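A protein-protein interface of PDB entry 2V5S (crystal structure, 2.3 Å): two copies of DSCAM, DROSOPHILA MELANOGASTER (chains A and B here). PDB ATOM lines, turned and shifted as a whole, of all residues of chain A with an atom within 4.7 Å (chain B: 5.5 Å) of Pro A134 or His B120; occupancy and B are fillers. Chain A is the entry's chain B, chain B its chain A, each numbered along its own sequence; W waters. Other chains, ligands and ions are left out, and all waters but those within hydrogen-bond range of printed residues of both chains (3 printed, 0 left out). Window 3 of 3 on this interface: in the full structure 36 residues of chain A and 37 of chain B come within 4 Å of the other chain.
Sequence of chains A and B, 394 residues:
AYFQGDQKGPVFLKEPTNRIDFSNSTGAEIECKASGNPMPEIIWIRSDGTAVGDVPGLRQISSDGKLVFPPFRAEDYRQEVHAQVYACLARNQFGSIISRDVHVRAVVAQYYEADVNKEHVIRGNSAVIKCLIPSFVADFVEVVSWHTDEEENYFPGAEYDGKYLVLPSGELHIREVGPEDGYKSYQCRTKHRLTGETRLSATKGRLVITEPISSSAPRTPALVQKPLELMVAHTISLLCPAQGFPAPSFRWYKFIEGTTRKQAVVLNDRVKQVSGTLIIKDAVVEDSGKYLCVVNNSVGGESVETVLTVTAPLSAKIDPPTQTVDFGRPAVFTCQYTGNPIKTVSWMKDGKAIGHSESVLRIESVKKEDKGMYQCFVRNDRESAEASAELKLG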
ATOM      1  N   GLU A 113      26.063  16.692  12.570  1.00  0.00           N
ATOM      2  CA  GLU A 113      25.980  18.155  12.638  1.00  0.00           C
ATOM      3  C   GLU A 113      24.650  18.538  13.291  1.00  0.00           C
ATOM      4  O   GLU A 113      23.652  17.839  13.191  1.00  0.00           O
ATOM      5  CB  GLU A 113      26.193  18.829  11.277  1.00  0.00           C
ATOM      6  CG  GLU A 113      25.175  18.286  10.260  1.00  0.00           C
ATOM      7  CD  GLU A 113      25.378  18.660   8.801  1.00  0.00           C
ATOM      8  OE1 GLU A 113      26.548  18.728   8.359  1.00  0.00           O
ATOM      9  OE2 GLU A 113      24.351  18.764   8.075  1.00  0.00           O
ATOM     10  N   ALA A 114      24.710  19.559  14.132  1.00  0.00           N
ATOM     11  CA  ALA A 114      23.541  20.241  14.635  1.00  0.00           C
ATOM     12  C   ALA A 114      23.098  21.337  13.654  1.00  0.00           C
ATOM     13  O   ALA A 114      23.846  21.885  12.840  1.00  0.00           O
ATOM     14  CB  ALA A 114      23.833  20.796  16.034  1.00  0.00           C
ATOM     15  N   ASP A 115      21.833  21.705  13.794  1.00  0.00           N
ATOM     16  CA  ASP A 115      21.284  22.791  12.995  1.00  0.00           C
ATOM     17  C   ASP A 115      20.484  23.774  13.838  1.00  0.00           C
ATOM     18  O   ASP A 115      19.993  23.430  14.911  1.00  0.00           O
ATOM     19  CB  ASP A 115      20.371  22.194  11.905  1.00  0.00           C
ATOM     20  CG  ASP A 115      21.160  21.433  10.844  1.00  0.00           C
ATOM     21  OD1 ASP A 115      22.045  22.052  10.216  1.00  0.00           O
ATOM     22  OD2 ASP A 115      20.940  20.209  10.696  1.00  0.00           O
ATOM     23  N   LEU A 132      18.895  21.833  16.879  1.00  0.00           N
ATOM     24  CA  LEU A 132      18.325  20.598  16.402  1.00  0.00           C
ATOM     25  C   LEU A 132      19.495  19.622  16.389  1.00  0.00           C
ATOM     26  O   LEU A 132      20.387  19.779  15.574  1.00  0.00           O
ATOM     27  CB  LEU A 132      17.701  20.866  15.011  1.00  0.00           C
ATOM     28  CG  LEU A 132      16.591  21.945  15.026  1.00  0.00           C
ATOM     29  CD1 LEU A 132      15.835  22.270  13.715  1.00  0.00           C
ATOM     30  CD2 LEU A 132      15.592  21.573  16.129  1.00  0.00           C
ATOM     31  N   ILE A 133      19.512  18.641  17.287  1.00  0.00           N
ATOM     32  CA  ILE A 133      20.486  17.565  17.276  1.00  0.00           C
ATOM     33  C   ILE A 133      19.794  16.298  16.794  1.00  0.00           C
ATOM     34  O   ILE A 133      18.815  15.915  17.427  1.00  0.00           O
ATOM     35  CB  ILE A 133      21.037  17.300  18.704  1.00  0.00           C
ATOM     36  CG1 ILE A 133      21.796  18.515  19.251  1.00  0.00           C
ATOM     37  CG2 ILE A 133      21.861  16.045  18.738  1.00  0.00           C
ATOM     38  CD1 ILE A 133      21.866  18.574  20.770  1.00  0.00           C
ATOM     39  N   PRO A 134      20.340  15.615  15.767  1.00  0.00           N
ATOM     40  CA  PRO A 134      19.877  14.327  15.234  1.00  0.00           C
ATOM     41  C   PRO A 134      19.593  13.232  16.246  1.00  0.00           C
ATOM     42  O   PRO A 134      20.491  12.831  16.976  1.00  0.00           O
ATOM     43  CB  PRO A 134      21.028  13.862  14.337  1.00  0.00           C
ATOM     44  CG  PRO A 134      21.751  15.074  13.963  1.00  0.00           C
ATOM     45  CD  PRO A 134      21.531  16.087  15.039  1.00  0.00           C
ATOM     46  N   SER A 135      18.365  12.750  16.307  1.00  0.00           N
ATOM     47  CA  SER A 135      17.958  11.729  17.283  1.00  0.00           C
ATOM     48  C   SER A 135      19.037  10.698  17.589  1.00  0.00           C
ATOM     49  O   SER A 135      19.330  10.409  18.755  1.00  0.00           O
ATOM     50  CB  SER A 135      16.683  10.975  16.857  1.00  0.00           C
ATOM     51  OG  SER A 135      16.909  10.127  15.742  1.00  0.00           O
ATOM     52  N   PHE A 136      19.641  10.146  16.544  1.00  0.00           N
ATOM     53  CA  PHE A 136      20.654   9.102  16.754  1.00  0.00           C
ATOM     54  C   PHE A 136      22.013   9.482  17.314  1.00  0.00           C
ATOM     55  O   PHE A 136      22.875   8.612  17.335  1.00  0.00           O
ATOM     56  CB  PHE A 136      20.933   8.293  15.491  1.00  0.00           C
ATOM     57  CG  PHE A 136      20.929   9.132  14.273  1.00  0.00           C
ATOM     58  CD1 PHE A 136      22.099   9.713  13.822  1.00  0.00           C
ATOM     59  CD2 PHE A 136      19.731   9.335  13.589  1.00  0.00           C
ATOM     60  CE1 PHE A 136      22.073  10.522  12.714  1.00  0.00           C
ATOM     61  CE2 PHE A 136      19.718  10.089  12.446  1.00  0.00           C
ATOM     62  CZ  PHE A 136      20.898  10.685  12.031  1.00  0.00           C
ATOM     63  N   VAL A 137      22.239  10.720  17.729  1.00  0.00           N
ATOM     64  CA  VAL A 137      23.402  11.057  18.545  1.00  0.00           C
ATOM     65  C   VAL A 137      22.991  11.860  19.781  1.00  0.00           C
ATOM     66  O   VAL A 137      23.807  12.150  20.664  1.00  0.00           O
ATOM     67  CB  VAL A 137      24.418  11.901  17.774  1.00  0.00           C
ATOM     68  CG1 VAL A 137      25.033  11.123  16.623  1.00  0.00           C
ATOM     69  CG2 VAL A 137      23.842  13.295  17.408  1.00  0.00           C
ATOM     70  N   ALA A 138      21.698  12.144  19.882  1.00  0.00           N
ATOM     71  CA  ALA A 138      21.111  12.976  20.929  1.00  0.00           C
ATOM     72  C   ALA A 138      21.306  12.437  22.341  1.00  0.00           C
ATOM     73  O   ALA A 138      21.253  13.238  23.265  1.00  0.00           O
ATOM     74  CB  ALA A 138      19.626  13.166  20.653  1.00  0.00           C
ATOM     75  N   LYS B 118      16.352  20.712   6.750  1.00  0.00           N
ATOM     76  CA  LYS B 118      17.114  19.470   6.702  1.00  0.00           C
ATOM     77  C   LYS B 118      16.506  18.430   7.629  1.00  0.00           C
ATOM     78  O   LYS B 118      16.205  18.772   8.779  1.00  0.00           O
ATOM     79  CB  LYS B 118      18.557  19.735   7.146  1.00  0.00           C
ATOM     80  CG  LYS B 118      19.250  20.680   6.189  1.00  0.00           C
ATOM     81  CD  LYS B 118      20.542  21.286   6.669  1.00  0.00           C
ATOM     82  CE  LYS B 118      21.517  20.202   6.951  1.00  0.00           C
ATOM     83  NZ  LYS B 118      22.602  20.815   7.758  1.00  0.00           N
ATOM     84  N   GLU B 119      16.414  17.188   7.147  1.00  0.00           N
ATOM     85  CA  GLU B 119      15.980  16.036   7.929  1.00  0.00           C
ATOM     86  C   GLU B 119      17.129  15.037   8.017  1.00  0.00           C
ATOM     87  O   GLU B 119      17.591  14.539   6.991  1.00  0.00           O
ATOM     88  CB  GLU B 119      14.810  15.389   7.173  1.00  0.00           C
ATOM     89  CG  GLU B 119      13.964  14.405   7.966  1.00  0.00           C
ATOM     90  CD  GLU B 119      13.301  15.031   9.194  1.00  0.00           C
ATOM     91  OE1 GLU B 119      13.093  16.277   9.237  1.00  0.00           O
ATOM     92  OE2 GLU B 119      12.973  14.209  10.093  1.00  0.00           O
ATOM     93  N   HIS B 120      17.666  14.799   9.210  1.00  0.00           N
ATOM     94  CA  HIS B 120      18.667  13.771   9.415  1.00  0.00           C
ATOM     95  C   HIS B 120      18.139  12.361   9.684  1.00  0.00           C
ATOM     96  O   HIS B 120      17.347  12.119  10.584  1.00  0.00           O
ATOM     97  CB  HIS B 120      19.628  14.142  10.553  1.00  0.00           C
ATOM     98  CG  HIS B 120      20.302  15.454  10.332  1.00  0.00           C
ATOM     99  ND1 HIS B 120      21.609  15.564   9.905  1.00  0.00           N
ATOM    100  CD2 HIS B 120      19.833  16.718  10.472  1.00  0.00           C
ATOM    101  CE1 HIS B 120      21.909  16.848   9.790  1.00  0.00           C
ATOM    102  NE2 HIS B 120      20.837  17.568  10.085  1.00  0.00           N
ATOM    103  N   VAL B 121      18.642  11.391   8.930  1.00  0.00           N
ATOM    104  CA  VAL B 121      18.127  10.044   9.004  1.00  0.00           C
ATOM    105  C   VAL B 121      19.215   9.021   8.743  1.00  0.00           C
ATOM    106  O   VAL B 121      20.199   9.250   8.061  1.00  0.00           O
ATOM    107  CB  VAL B 121      16.947   9.879   8.004  1.00  0.00           C
ATOM    108  CG1 VAL B 121      15.908  10.952   8.292  1.00  0.00           C
ATOM    109  CG2 VAL B 121      17.439   9.992   6.567  1.00  0.00           C
ATOM    110  N   ILE B 122      19.002   7.848   9.314  1.00  0.00           N
ATOM    111  CA  ILE B 122      19.902   6.703   9.216  1.00  0.00           C
ATOM    112  C   ILE B 122      19.480   5.958   7.953  1.00  0.00           C
ATOM    113  O   ILE B 122      18.297   5.671   7.813  1.00  0.00           O
ATOM    114  CB  ILE B 122      19.709   5.774  10.437  1.00  0.00           C
ATOM    115  CG1 ILE B 122      20.102   6.494  11.736  1.00  0.00           C
ATOM    116  CG2 ILE B 122      20.596   4.521  10.336  1.00  0.00           C
ATOM    117  CD1 ILE B 122      20.236   5.600  12.968  1.00  0.00           C
ATOM    118  N   ARG B 206      16.518  19.143   2.598  1.00  0.00           N
ATOM    119  CA  ARG B 206      17.200  17.948   2.101  1.00  0.00           C
ATOM    120  C   ARG B 206      17.235  16.916   3.231  1.00  0.00           C
ATOM    121  O   ARG B 206      16.993  17.249   4.387  1.00  0.00           O
ATOM    122  CB  ARG B 206      18.570  18.321   1.528  1.00  0.00           C
ATOM    123  CG  ARG B 206      19.471  19.075   2.515  1.00  0.00           C
ATOM    124  CD  ARG B 206      20.610  19.768   1.776  1.00  0.00           C
ATOM    125  NE  ARG B 206      21.717  20.344   2.551  1.00  0.00           N
ATOM    126  CZ  ARG B 206      22.718  19.656   3.081  1.00  0.00           C
ATOM    127  NH1 ARG B 206      22.694  18.335   3.003  1.00  0.00           N
ATOM    128  NH2 ARG B 206      23.727  20.270   3.694  1.00  0.00           N
ATOM    129  N   LEU B 207      17.394  15.643   2.887  1.00  0.00           N
ATOM    130  CA  LEU B 207      17.650  14.514   3.776  1.00  0.00           C
ATOM    131  C   LEU B 207      19.158  14.469   3.861  1.00  0.00           C
ATOM    132  O   LEU B 207      19.767  14.528   2.789  1.00  0.00           O
ATOM    133  CB  LEU B 207      17.225  13.208   3.111  1.00  0.00           C
ATOM    134  CG  LEU B 207      15.738  12.938   2.857  1.00  0.00           C
ATOM    135  CD1 LEU B 207      15.505  11.594   2.170  1.00  0.00           C
ATOM    136  CD2 LEU B 207      15.131  12.939   4.251  1.00  0.00           C
ATOM    137  N   VAL B 208      19.712  14.492   5.075  1.00  0.00           N
ATOM    138  CA  VAL B 208      21.121  14.191   5.336  1.00  0.00           C
ATOM    139  C   VAL B 208      21.179  12.795   5.957  1.00  0.00           C
ATOM    140  O   VAL B 208      20.638  12.525   7.037  1.00  0.00           O
ATOM    141  CB  VAL B 208      21.821  15.227   6.250  1.00  0.00           C
ATOM    142  CG1 VAL B 208      23.369  15.133   6.165  1.00  0.00           C
ATOM    143  CG2 VAL B 208      21.361  16.633   5.862  1.00  0.00           C
ATOM    144  N   GLN B 243      14.079   6.439  14.670  1.00  0.00           N
ATOM    145  CA  GLN B 243      15.240   6.141  13.846  1.00  0.00           C
ATOM    146  C   GLN B 243      16.044   5.115  14.628  1.00  0.00           C
ATOM    147  O   GLN B 243      16.324   5.266  15.814  1.00  0.00           O
ATOM    148  CB  GLN B 243      16.089   7.386  13.611  1.00  0.00           C
ATOM    149  CG  GLN B 243      15.597   8.509  12.688  1.00  0.00           C
ATOM    150  CD  GLN B 243      15.537   8.033  11.261  1.00  0.00           C
ATOM    151  OE1 GLN B 243      14.491   8.027  10.592  1.00  0.00           O
ATOM    152  NE2 GLN B 243      16.698   7.672  10.762  1.00  0.00           N
HETATM  153  O   HOH W   1      17.063  13.122  13.636  1.00  0.00           O
HETATM  154  O   HOH W   2      19.726  18.399  13.211  1.00  0.00           O
HETATM  155  O   HOH W   3      24.151  14.781  11.092  1.00  0.00           O
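Pro A134 touches just one residue of chain B: His B120.
His B120 touches four residues of chain A.
Printed residues of chain B within 4 Å of Glu A113: Lys B118 (2.7 Å) and His B120 (3.5 Å).
Printed residues of chain A within 4 Å of Gln B243: Ser A135.
Printed residues of chain B within 4 Å of Ser A135: Gln B243.
Printed residues of chain A within 4 Å of Ile B122: Phe A136.
Of the printed residues of chain A, Lys B118 touches Glu A113 (2.7 Å) and Asp A115 (2.8 Å).
The nearest printed residue of chain B that does not touch Pro A134 is Val B121 (6.4 Å).
The nearest printed residue of chain A that does not touch His B120 is Ser A135 (5.5 Å).
O of Asp A115 sits at hydrogen-bond distance from N of Leu A132 (2.8 Å).
The side-chain amide nitrogen of Gln B243 sits close to the backbone NH of Ile B122.
The backbone carbonyl oxygen (O) of Val B208 is in hydrogen-bond range of the backbone NH (N) of Val B121, 3.0 Å away.
Of the 9 printed residues of chain B, 5 touch a printed residue of chain A.
Among the printed residues, Asp or Glu carboxylates within 4 Å of a Lys or Arg side-chain nitrogen of the other chain: Glu A113 with Lys B118 and Asp A115 with Lys B118.
Among the printed residues, pairs that only touch across the chains: Glu A113 with His B120 (3.5 Å), Pro A134 with His B120 (3.9 Å), Ser A135 with Gln B243 (3.6 Å), Phe A136 with His B120 (3.6 Å), Phe A136 with Val B121 (3.8 Å) and Phe A136 with Ile B122 (3.4 Å).
No position is printed for both chains.
Of the 9 pairs that touch across the chains among the printed residues, none has its exchanged pair printed and touching as well.
Water W2 lies within hydrogen-bond range of O of Leu A132 (2.8 Å), OD2 of Asp A115 (3.3 Å) and NE2 of His B120 (3.4 Å).
Water W3 lies within hydrogen-bond range of ND1 of His B120 (2.9 Å) and N of Glu A113 (3.1 Å).
Water W1 bridges N of Ser A135 (3.0 Å) and O of His B120 (3.2 Å).
NE2 of His B120 is in hydrogen-bond range of OD2 of Asp A115 (2.7 Å).
The side-chain carboxylate of Asp A115 is in salt-bridge range of the side-chain amino group of Lys B118 (2.8 Å).
The side-chain carboxylate (OE2) of Glu A113 lies within salt-bridge range of the side-chain amino group (NZ) of Lys B118 (2.7 Å).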
